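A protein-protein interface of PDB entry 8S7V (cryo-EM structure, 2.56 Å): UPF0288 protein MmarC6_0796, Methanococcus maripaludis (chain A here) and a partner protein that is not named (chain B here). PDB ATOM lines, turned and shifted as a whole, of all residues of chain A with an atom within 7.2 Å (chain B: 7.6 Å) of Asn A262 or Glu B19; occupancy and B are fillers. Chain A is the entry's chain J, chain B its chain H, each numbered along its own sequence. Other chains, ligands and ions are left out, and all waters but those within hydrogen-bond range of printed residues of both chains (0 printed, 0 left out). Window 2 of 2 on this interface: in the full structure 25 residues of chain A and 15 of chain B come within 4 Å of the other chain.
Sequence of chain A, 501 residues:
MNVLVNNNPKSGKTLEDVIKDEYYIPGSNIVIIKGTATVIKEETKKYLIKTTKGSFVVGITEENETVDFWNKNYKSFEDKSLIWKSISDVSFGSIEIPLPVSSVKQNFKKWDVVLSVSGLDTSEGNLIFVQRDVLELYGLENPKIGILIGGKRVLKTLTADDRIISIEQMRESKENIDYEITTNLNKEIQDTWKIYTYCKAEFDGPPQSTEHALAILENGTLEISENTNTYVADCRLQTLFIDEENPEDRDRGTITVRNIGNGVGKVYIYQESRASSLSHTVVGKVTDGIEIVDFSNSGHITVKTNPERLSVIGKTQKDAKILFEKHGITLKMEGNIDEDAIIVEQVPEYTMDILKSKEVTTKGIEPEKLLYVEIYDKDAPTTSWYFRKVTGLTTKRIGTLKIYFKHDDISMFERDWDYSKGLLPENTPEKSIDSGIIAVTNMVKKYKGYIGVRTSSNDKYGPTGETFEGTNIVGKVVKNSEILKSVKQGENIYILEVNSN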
ATOM      1  N   TYR A 231      21.054 -15.978  -8.604  1.00  0.00           N
ATOM      2  CA  TYR A 231      21.840 -14.769  -8.422  1.00  0.00           C
ATOM      3  C   TYR A 231      23.242 -15.115  -7.941  1.00  0.00           C
ATOM      4  O   TYR A 231      23.536 -16.247  -7.554  1.00  0.00           O
ATOM      5  CB  TYR A 231      21.171 -13.802  -7.432  1.00  0.00           C
ATOM      6  CG  TYR A 231      21.151 -14.285  -5.995  1.00  0.00           C
ATOM      7  CD1 TYR A 231      22.240 -14.085  -5.157  1.00  0.00           C
ATOM      8  CD2 TYR A 231      20.040 -14.932  -5.476  1.00  0.00           C
ATOM      9  CE1 TYR A 231      22.226 -14.524  -3.850  1.00  0.00           C
ATOM     10  CE2 TYR A 231      20.017 -15.373  -4.169  1.00  0.00           C
ATOM     11  CZ  TYR A 231      21.113 -15.165  -3.361  1.00  0.00           C
ATOM     12  OH  TYR A 231      21.098 -15.600  -2.057  1.00  0.00           O
ATOM     13  N   GLN A 238      28.664  -5.377   3.664  1.00  0.00           N
ATOM     14  CA  GLN A 238      27.453  -6.027   4.138  1.00  0.00           C
ATOM     15  C   GLN A 238      26.881  -5.357   5.384  1.00  0.00           C
ATOM     16  O   GLN A 238      25.740  -5.636   5.762  1.00  0.00           O
ATOM     17  CB  GLN A 238      27.744  -7.520   4.388  1.00  0.00           C
ATOM     18  CG  GLN A 238      26.833  -8.253   5.363  1.00  0.00           C
ATOM     19  CD  GLN A 238      26.384  -9.602   4.848  1.00  0.00           C
ATOM     20  OE1 GLN A 238      27.011 -10.182   3.965  1.00  0.00           O
ATOM     21  NE2 GLN A 238      25.288 -10.109   5.398  1.00  0.00           N
ATOM     22  N   THR A 239      27.620  -4.437   5.999  1.00  0.00           N
ATOM     23  CA  THR A 239      27.147  -3.767   7.204  1.00  0.00           C
ATOM     24  C   THR A 239      27.017  -2.263   6.992  1.00  0.00           C
ATOM     25  O   THR A 239      26.922  -1.501   7.957  1.00  0.00           O
ATOM     26  CB  THR A 239      28.063  -4.067   8.388  1.00  0.00           C
ATOM     27  OG1 THR A 239      29.428  -4.043   7.956  1.00  0.00           O
ATOM     28  CG2 THR A 239      27.745  -5.436   8.964  1.00  0.00           C
ATOM     29  N   ARG A 250      13.387  -7.625 -11.034  1.00  0.00           N
ATOM     30  CA  ARG A 250      14.762  -8.120 -11.021  1.00  0.00           C
ATOM     31  C   ARG A 250      14.933  -9.059 -12.212  1.00  0.00           C
ATOM     32  O   ARG A 250      14.921 -10.285 -12.092  1.00  0.00           O
ATOM     33  CB  ARG A 250      15.070  -8.812  -9.701  1.00  0.00           C
ATOM     34  CG  ARG A 250      14.946  -7.910  -8.487  1.00  0.00           C
ATOM     35  CD  ARG A 250      15.133  -8.689  -7.199  1.00  0.00           C
ATOM     36  NE  ARG A 250      13.960  -9.489  -6.870  1.00  0.00           N
ATOM     37  CZ  ARG A 250      13.897 -10.346  -5.861  1.00  0.00           C
ATOM     38  NH1 ARG A 250      14.930 -10.547  -5.060  1.00  0.00           N
ATOM     39  NH2 ARG A 250      12.770 -11.019  -5.651  1.00  0.00           N
ATOM     40  N   ARG A 258      20.805  -4.818  -1.604  1.00  0.00           N
ATOM     41  CA  ARG A 258      19.865  -5.059  -0.518  1.00  0.00           C
ATOM     42  C   ARG A 258      19.973  -3.932   0.500  1.00  0.00           C
ATOM     43  O   ARG A 258      21.064  -3.632   0.992  1.00  0.00           O
ATOM     44  CB  ARG A 258      20.143  -6.408   0.141  1.00  0.00           C
ATOM     45  CG  ARG A 258      19.262  -6.709   1.335  1.00  0.00           C
ATOM     46  CD  ARG A 258      19.409  -8.154   1.770  1.00  0.00           C
ATOM     47  NE  ARG A 258      18.317  -8.985   1.280  1.00  0.00           N
ATOM     48  CZ  ARG A 258      17.129  -9.076   1.860  1.00  0.00           C
ATOM     49  NH1 ARG A 258      16.844  -8.397   2.957  1.00  0.00           N
ATOM     50  NH2 ARG A 258      16.206  -9.868   1.324  1.00  0.00           N
ATOM     51  N   ILE A 260      17.984  -3.523   3.425  1.00  0.00           N
ATOM     52  CA  ILE A 260      17.432  -3.777   4.748  1.00  0.00           C
ATOM     53  C   ILE A 260      17.708  -5.225   5.122  1.00  0.00           C
ATOM     54  O   ILE A 260      17.798  -6.103   4.260  1.00  0.00           O
ATOM     55  CB  ILE A 260      15.918  -3.460   4.802  1.00  0.00           C
ATOM     56  CG1 ILE A 260      15.448  -3.322   6.251  1.00  0.00           C
ATOM     57  CG2 ILE A 260      15.111  -4.525   4.076  1.00  0.00           C
ATOM     58  CD1 ILE A 260      16.162  -2.230   7.019  1.00  0.00           C
ATOM     59  N   GLY A 261      17.876  -5.465   6.413  1.00  0.00           N
ATOM     60  CA  GLY A 261      18.006  -6.802   6.943  1.00  0.00           C
ATOM     61  C   GLY A 261      19.426  -7.137   7.352  1.00  0.00           C
ATOM     62  O   GLY A 261      20.283  -6.268   7.527  1.00  0.00           O
ATOM     63  N   ASN A 262      19.668  -8.439   7.514  1.00  0.00           N
ATOM     64  CA  ASN A 262      21.003  -8.905   7.871  1.00  0.00           C
ATOM     65  C   ASN A 262      22.008  -8.646   6.759  1.00  0.00           C
ATOM     66  O   ASN A 262      23.188  -8.401   7.035  1.00  0.00           O
ATOM     67  CB  ASN A 262      20.965 -10.394   8.211  1.00  0.00           C
ATOM     68  CG  ASN A 262      22.234 -10.870   8.889  1.00  0.00           C
ATOM     69  OD1 ASN A 262      23.011 -11.629   8.313  1.00  0.00           O
ATOM     70  ND2 ASN A 262      22.448 -10.426  10.122  1.00  0.00           N
ATOM     71  N   GLY A 263      21.568  -8.691   5.504  1.00  0.00           N
ATOM     72  CA  GLY A 263      22.469  -8.510   4.385  1.00  0.00           C
ATOM     73  C   GLY A 263      22.327  -7.169   3.696  1.00  0.00           C
ATOM     74  O   GLY A 263      22.382  -7.091   2.466  1.00  0.00           O
ATOM     75  N   VAL A 264      22.150  -6.104   4.477  1.00  0.00           N
ATOM     76  CA  VAL A 264      22.000  -4.773   3.905  1.00  0.00           C
ATOM     77  C   VAL A 264      23.324  -4.329   3.297  1.00  0.00           C
ATOM     78  O   VAL A 264      24.363  -4.318   3.965  1.00  0.00           O
ATOM     79  CB  VAL A 264      21.510  -3.781   4.971  1.00  0.00           C
ATOM     80  CG1 VAL A 264      22.301  -3.942   6.259  1.00  0.00           C
ATOM     81  CG2 VAL A 264      21.613  -2.357   4.457  1.00  0.00           C
ATOM     82  N   GLY A 265      23.292  -3.957   2.023  1.00  0.00           N
ATOM     83  CA  GLY A 265      24.480  -3.521   1.324  1.00  0.00           C
ATOM     84  C   GLY A 265      25.087  -4.547   0.394  1.00  0.00           C
ATOM     85  O   GLY A 265      25.993  -4.200  -0.373  1.00  0.00           O
ATOM     86  N   LYS A 266      24.629  -5.795   0.443  1.00  0.00           N
ATOM     87  CA  LYS A 266      25.090  -6.792  -0.510  1.00  0.00           C
ATOM     88  C   LYS A 266      24.663  -6.408  -1.919  1.00  0.00           C
ATOM     89  O   LYS A 266      23.568  -5.882  -2.130  1.00  0.00           O
ATOM     90  CB  LYS A 266      24.535  -8.170  -0.157  1.00  0.00           C
ATOM     91  CG  LYS A 266      25.288  -8.889   0.938  1.00  0.00           C
ATOM     92  CD  LYS A 266      24.398  -9.916   1.607  1.00  0.00           C
ATOM     93  CE  LYS A 266      24.247 -11.149   0.736  1.00  0.00           C
ATOM     94  NZ  LYS A 266      23.273 -12.118   1.306  1.00  0.00           N
ATOM     95  N   TYR A 268      23.777  -7.730  -5.617  1.00  0.00           N
ATOM     96  CA  TYR A 268      23.297  -8.925  -6.292  1.00  0.00           C
ATOM     97  C   TYR A 268      23.315  -8.719  -7.799  1.00  0.00           C
ATOM     98  O   TYR A 268      23.052  -7.616  -8.287  1.00  0.00           O
ATOM     99  CB  TYR A 268      21.873  -9.276  -5.853  1.00  0.00           C
ATOM    100  CG  TYR A 268      21.719  -9.617  -4.392  1.00  0.00           C
ATOM    101  CD1 TYR A 268      21.645  -8.621  -3.429  1.00  0.00           C
ATOM    102  CD2 TYR A 268      21.625 -10.935  -3.976  1.00  0.00           C
ATOM    103  CE1 TYR A 268      21.497  -8.932  -2.095  1.00  0.00           C
ATOM    104  CE2 TYR A 268      21.477 -11.254  -2.646  1.00  0.00           C
ATOM    105  CZ  TYR A 268      21.413 -10.249  -1.709  1.00  0.00           C
ATOM    106  OH  TYR A 268      21.264 -10.565  -0.380  1.00  0.00           O
ATOM    107  N   SER A 279      12.965  -5.107  -0.662  1.00  0.00           N
ATOM    108  CA  SER A 279      14.242  -5.134   0.035  1.00  0.00           C
ATOM    109  C   SER A 279      15.434  -5.055  -0.907  1.00  0.00           C
ATOM    110  O   SER A 279      16.576  -5.122  -0.442  1.00  0.00           O
ATOM    111  CB  SER A 279      14.353  -6.401   0.886  1.00  0.00           C
ATOM    112  OG  SER A 279      13.126  -6.688   1.531  1.00  0.00           O
ATOM    113  N   HIS A 280      15.203  -4.919  -2.210  1.00  0.00           N
ATOM    114  CA  HIS A 280      16.273  -4.847  -3.194  1.00  0.00           C
ATOM    115  C   HIS A 280      16.159  -3.541  -3.964  1.00  0.00           C
ATOM    116  O   HIS A 280      15.105  -3.240  -4.533  1.00  0.00           O
ATOM    117  CB  HIS A 280      16.219  -6.038  -4.152  1.00  0.00           C
ATOM    118  CG  HIS A 280      16.726  -7.312  -3.555  1.00  0.00           C
ATOM    119  ND1 HIS A 280      18.001  -7.783  -3.779  1.00  0.00           N
ATOM    120  CD2 HIS A 280      16.132  -8.212  -2.737  1.00  0.00           C
ATOM    121  CE1 HIS A 280      18.169  -8.920  -3.128  1.00  0.00           C
ATOM    122  NE2 HIS A 280      17.050  -9.202  -2.487  1.00  0.00           N
ATOM    123  N   LYS B  13      16.540 -17.149  14.058  1.00  0.00           N
ATOM    124  CA  LYS B  13      17.186 -17.006  12.752  1.00  0.00           C
ATOM    125  C   LYS B  13      16.227 -17.301  11.603  1.00  0.00           C
ATOM    126  O   LYS B  13      16.653 -17.646  10.498  1.00  0.00           O
ATOM    127  CB  LYS B  13      18.432 -17.890  12.644  1.00  0.00           C
ATOM    128  CG  LYS B  13      19.435 -17.686  13.761  1.00  0.00           C
ATOM    129  CD  LYS B  13      20.856 -17.815  13.250  1.00  0.00           C
ATOM    130  CE  LYS B  13      21.467 -19.143  13.660  1.00  0.00           C
ATOM    131  NZ  LYS B  13      22.423 -18.990  14.788  1.00  0.00           N
ATOM    132  N   ASN B  14      14.923 -17.165  11.845  1.00  0.00           N
ATOM    133  CA  ASN B  14      13.950 -17.340  10.775  1.00  0.00           C
ATOM    134  C   ASN B  14      13.933 -16.148   9.828  1.00  0.00           C
ATOM    135  O   ASN B  14      13.599 -16.301   8.646  1.00  0.00           O
ATOM    136  CB  ASN B  14      12.558 -17.566  11.364  1.00  0.00           C
ATOM    137  CG  ASN B  14      11.554 -18.015  10.328  1.00  0.00           C
ATOM    138  OD1 ASN B  14      11.793 -18.969   9.589  1.00  0.00           O
ATOM    139  ND2 ASN B  14      10.420 -17.331  10.268  1.00  0.00           N
ATOM    140  N   ASN B  15      14.292 -14.963  10.326  1.00  0.00           N
ATOM    141  CA  ASN B  15      14.347 -13.782   9.473  1.00  0.00           C
ATOM    142  C   ASN B  15      15.420 -13.913   8.400  1.00  0.00           C
ATOM    143  O   ASN B  15      15.226 -13.442   7.275  1.00  0.00           O
ATOM    144  CB  ASN B  15      14.583 -12.535  10.323  1.00  0.00           C
ATOM    145  CG  ASN B  15      15.877 -12.602  11.107  1.00  0.00           C
ATOM    146  OD1 ASN B  15      16.011 -13.394  12.038  1.00  0.00           O
ATOM    147  ND2 ASN B  15      16.836 -11.766  10.734  1.00  0.00           N
ATOM    148  N   ILE B  16      16.548 -14.553   8.717  1.00  0.00           N
ATOM    149  CA  ILE B  16      17.581 -14.763   7.708  1.00  0.00           C
ATOM    150  C   ILE B  16      17.082 -15.712   6.624  1.00  0.00           C
ATOM    151  O   ILE B  16      17.354 -15.517   5.433  1.00  0.00           O
ATOM    152  CB  ILE B  16      18.876 -15.272   8.366  1.00  0.00           C
ATOM    153  CG1 ILE B  16      19.489 -14.187   9.250  1.00  0.00           C
ATOM    154  CG2 ILE B  16      19.887 -15.671   7.311  1.00  0.00           C
ATOM    155  CD1 ILE B  16      19.210 -14.366  10.722  1.00  0.00           C
ATOM    156  N   LEU B  17      16.340 -16.751   7.015  1.00  0.00           N
ATOM    157  CA  LEU B  17      15.755 -17.650   6.025  1.00  0.00           C
ATOM    158  C   LEU B  17      14.735 -16.928   5.154  1.00  0.00           C
ATOM    159  O   LEU B  17      14.663 -17.167   3.942  1.00  0.00           O
ATOM    160  CB  LEU B  17      15.114 -18.852   6.715  1.00  0.00           C
ATOM    161  CG  LEU B  17      14.528 -19.912   5.782  1.00  0.00           C
ATOM    162  CD1 LEU B  17      15.616 -20.825   5.247  1.00  0.00           C
ATOM    163  CD2 LEU B  17      13.458 -20.716   6.495  1.00  0.00           C
ATOM    164  N   LYS B  18      13.930 -16.047   5.752  1.00  0.00           N
ATOM    165  CA  LYS B  18      12.992 -15.257   4.959  1.00  0.00           C
ATOM    166  C   LYS B  18      13.731 -14.341   3.992  1.00  0.00           C
ATOM    167  O   LYS B  18      13.291 -14.140   2.854  1.00  0.00           O
ATOM    168  CB  LYS B  18      12.076 -14.452   5.877  1.00  0.00           C
ATOM    169  CG  LYS B  18      11.100 -15.304   6.666  1.00  0.00           C
ATOM    170  CD  LYS B  18       9.684 -14.773   6.552  1.00  0.00           C
ATOM    171  CE  LYS B  18       9.445 -13.626   7.513  1.00  0.00           C
ATOM    172  NZ  LYS B  18       9.211 -14.114   8.896  1.00  0.00           N
ATOM    173  N   GLU B  19      14.858 -13.775   4.429  1.00  0.00           N
ATOM    174  CA  GLU B  19      15.678 -12.963   3.536  1.00  0.00           C
ATOM    175  C   GLU B  19      16.214 -13.792   2.376  1.00  0.00           C
ATOM    176  O   GLU B  19      16.246 -13.325   1.235  1.00  0.00           O
ATOM    177  CB  GLU B  19      16.831 -12.331   4.312  1.00  0.00           C
ATOM    178  CG  GLU B  19      16.426 -11.160   5.182  1.00  0.00           C
ATOM    179  CD  GLU B  19      17.603 -10.559   5.918  1.00  0.00           C
ATOM    180  OE1 GLU B  19      18.729 -10.621   5.386  1.00  0.00           O
ATOM    181  OE2 GLU B  19      17.403 -10.029   7.032  1.00  0.00           O
ATOM    182  N   TRP B  20      16.649 -15.022   2.654  1.00  0.00           N
ATOM    183  CA  TRP B  20      17.114 -15.905   1.586  1.00  0.00           C
ATOM    184  C   TRP B  20      15.993 -16.211   0.599  1.00  0.00           C
ATOM    185  O   TRP B  20      16.207 -16.211  -0.620  1.00  0.00           O
ATOM    186  CB  TRP B  20      17.667 -17.198   2.184  1.00  0.00           C
ATOM    187  CG  TRP B  20      18.316 -18.108   1.187  1.00  0.00           C
ATOM    188  CD1 TRP B  20      19.642 -18.171   0.876  1.00  0.00           C
ATOM    189  CD2 TRP B  20      17.669 -19.100   0.381  1.00  0.00           C
ATOM    190  NE1 TRP B  20      19.860 -19.133  -0.078  1.00  0.00           N
ATOM    191  CE2 TRP B  20      18.664 -19.718  -0.399  1.00  0.00           C
ATOM    192  CE3 TRP B  20      16.343 -19.521   0.240  1.00  0.00           C
ATOM    193  CZ2 TRP B  20      18.378 -20.734  -1.305  1.00  0.00           C
ATOM    194  CZ3 TRP B  20      16.061 -20.529  -0.662  1.00  0.00           C
ATOM    195  CH2 TRP B  20      17.073 -21.125  -1.422  1.00  0.00           C
ATOM    196  N   ILE B  21      14.792 -16.475   1.114  1.00  0.00           N
ATOM    197  CA  ILE B  21      13.650 -16.762   0.249  1.00  0.00           C
ATOM    198  C   ILE B  21      13.331 -15.559  -0.630  1.00  0.00           C
ATOM    199  O   ILE B  21      13.050 -15.702  -1.826  1.00  0.00           O
ATOM    200  CB  ILE B  21      12.437 -17.188   1.095  1.00  0.00           C
ATOM    201  CG1 ILE B  21      12.643 -18.596   1.649  1.00  0.00           C
ATOM    202  CG2 ILE B  21      11.162 -17.122   0.277  1.00  0.00           C
ATOM    203  CD1 ILE B  21      11.772 -18.912   2.839  1.00  0.00           C
ATOM    204  N   GLU B  22      13.366 -14.357  -0.052  1.00  0.00           N
ATOM    205  CA  GLU B  22      13.147 -13.148  -0.840  1.00  0.00           C
ATOM    206  C   GLU B  22      14.240 -12.961  -1.884  1.00  0.00           C
ATOM    207  O   GLU B  22      13.964 -12.529  -3.009  1.00  0.00           O
ATOM    208  CB  GLU B  22      13.077 -11.930   0.079  1.00  0.00           C
ATOM    209  CG  GLU B  22      11.823 -11.863   0.930  1.00  0.00           C
ATOM    210  CD  GLU B  22      11.934 -10.839   2.044  1.00  0.00           C
ATOM    211  OE1 GLU B  22      11.089 -10.864   2.964  1.00  0.00           O
ATOM    212  OE2 GLU B  22      12.868 -10.011   1.999  1.00  0.00           O
ATOM    213  N   ASP B  23      15.489 -13.267  -1.524  1.00  0.00           N
ATOM    214  CA  ASP B  23      16.595 -13.116  -2.463  1.00  0.00           C
ATOM    215  C   ASP B  23      16.437 -14.042  -3.661  1.00  0.00           C
ATOM    216  O   ASP B  23      16.644 -13.623  -4.805  1.00  0.00           O
ATOM    217  CB  ASP B  23      17.923 -13.384  -1.756  1.00  0.00           C
ATOM    218  CG  ASP B  23      18.330 -12.255  -0.833  1.00  0.00           C
ATOM    219  OD1 ASP B  23      17.707 -11.176  -0.899  1.00  0.00           O
ATOM    220  OD2 ASP B  23      19.277 -12.445  -0.042  1.00  0.00           O
ATOM    221  N   VAL B  24      16.070 -15.305  -3.423  1.00  0.00           N
ATOM    222  CA  VAL B  24      15.916 -16.250  -4.529  1.00  0.00           C
ATOM    223  C   VAL B  24      14.600 -16.084  -5.265  1.00  0.00           C
ATOM    224  O   VAL B  24      14.356 -16.809  -6.239  1.00  0.00           O
ATOM    225  CB  VAL B  24      16.038 -17.711  -4.053  1.00  0.00           C
ATOM    226  CG1 VAL B  24      17.336 -17.911  -3.294  1.00  0.00           C
ATOM    227  CG2 VAL B  24      14.846 -18.094  -3.200  1.00  0.00           C
ATOM    228  N   GLY B  25      13.746 -15.159  -4.840  1.00  0.00           N
ATOM    229  CA  GLY B  25      12.519 -14.874  -5.551  1.00  0.00           C
ATOM    230  C   GLY B  25      11.288 -15.603  -5.067  1.00  0.00           C
ATOM    231  O   GLY B  25      10.254 -15.549  -5.742  1.00  0.00           O
ATOM    232  N   ILE B  28       6.351 -15.881   0.604  1.00  0.00           N
ATOM    233  CA  ILE B  28       5.846 -16.486   1.831  1.00  0.00           C
ATOM    234  C   ILE B  28       4.331 -16.332   1.822  1.00  0.00           C
ATOM    235  O   ILE B  28       3.803 -15.253   2.104  1.00  0.00           O
ATOM    236  CB  ILE B  28       6.470 -15.847   3.076  1.00  0.00           C
ATOM    237  CG1 ILE B  28       7.956 -16.196   3.162  1.00  0.00           C
ATOM    238  CG2 ILE B  28       5.766 -16.325   4.331  1.00  0.00           C
ATOM    239  CD1 ILE B  28       8.875 -15.057   2.787  1.00  0.00           C
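OE2 of Glu B22 is in salt-bridge range of NH2 of Arg A258.
The side-chain carboxylate (OE1) of Glu B19 is in hydrogen-bond range of the backbone NH (N) of Gly A263 (3.4 Å).
The side-chain carboxylate (OE2) of Glu B22 sits at hydrogen-bond distance from the side-chain hydroxyl (OG) of Ser A279.
NH1 of Arg A258 is in salt-bridge range of OE1 of Glu B19.
The guanidinium group (NH2) of Arg A258 lies within salt-bridge range of the side-chain carboxylate (OD1) of Asp B23 (3.0 Å).
The side-chain hydroxyl (OH) of Tyr A268 lies within hydrogen-bond range of the side-chain carboxylate (OD2) of Asp B23 (2.8 Å).
A ring nitrogen (NE2) of His A280 lies within hydrogen-bond range of the side-chain carboxylate (OD1) of Asp B23, at 2.6 Å.
The backbone carbonyl oxygen of Glu B22 is in hydrogen-bond range of the guanidinium group of Arg A250 (3.0 Å).
The side-chain carboxylate (OE2) of Glu B19 is in hydrogen-bond range of the backbone NH (N) of Asn A262, 2.8 Å away.
The side-chain amino group of Lys A266 is in hydrogen-bond range of the side-chain hydroxyl of Tyr A268, at 3.0 Å.
N of Arg A258 lies within hydrogen-bond range of O of Lys A266 (3.0 Å).
NH1 of Arg A258 lies within hydrogen-bond range of O of Ile A260 (2.8 Å).
NE2 of Gln A238 sits at hydrogen-bond distance from O of Asn A262 (3.2 Å).
N of Gly A265 is in hydrogen-bond range of O of Arg A258, at 2.5 Å.
Among the printed residues, pairs that only touch across the chains: Gly A261 with Glu B19 (3.3 Å), Arg A250 with Asp B23 (3.5 Å), Tyr A231 with Asp B23 (3.7 Å), Tyr A231 with Val B24 (3.8 Å) and Arg A250 with Gly B25 (3.9 Å).
Of chain B, only Glu B19 (2.8 Å) comes within 4 Å of Asn A262.
Of the printed residues of chain B, Gly A263 touches Glu B19 (3.4 Å).
Printed residues of chain A within 4 Å of Asp B23: Tyr A231, Arg A250, Arg A258, Tyr A268 and His A280.
Printed residues of chain B within 4 Å of Tyr A231: Asp B23 and Val B24.
Of the printed residues of chain B, Ser A279 touches Glu B22 (3.4 Å).
The nearest residue of chain B that does not touch Asn A262 is Ile B16 (4.2 Å).
The nearest residue of chain A that does not touch Glu B19 is Ile A260 (4.7 Å).
Of the 14 printed residues of chain B, 5 touch a printed residue of chain A.
Hydrophobic or aromatic side chains of chain A within 4 Å of the printed part of chain B: Tyr A231, Tyr A268 and His A280.
Among the printed residues, Asp or Glu carboxylates within 4 Å of a Lys or Arg side-chain nitrogen of the other chain: Arg A258 with Glu B19 (3.8 Å), Arg A258 with Glu B22 (3.4 Å) and Arg A258 with Asp B23 (3.0 Å).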
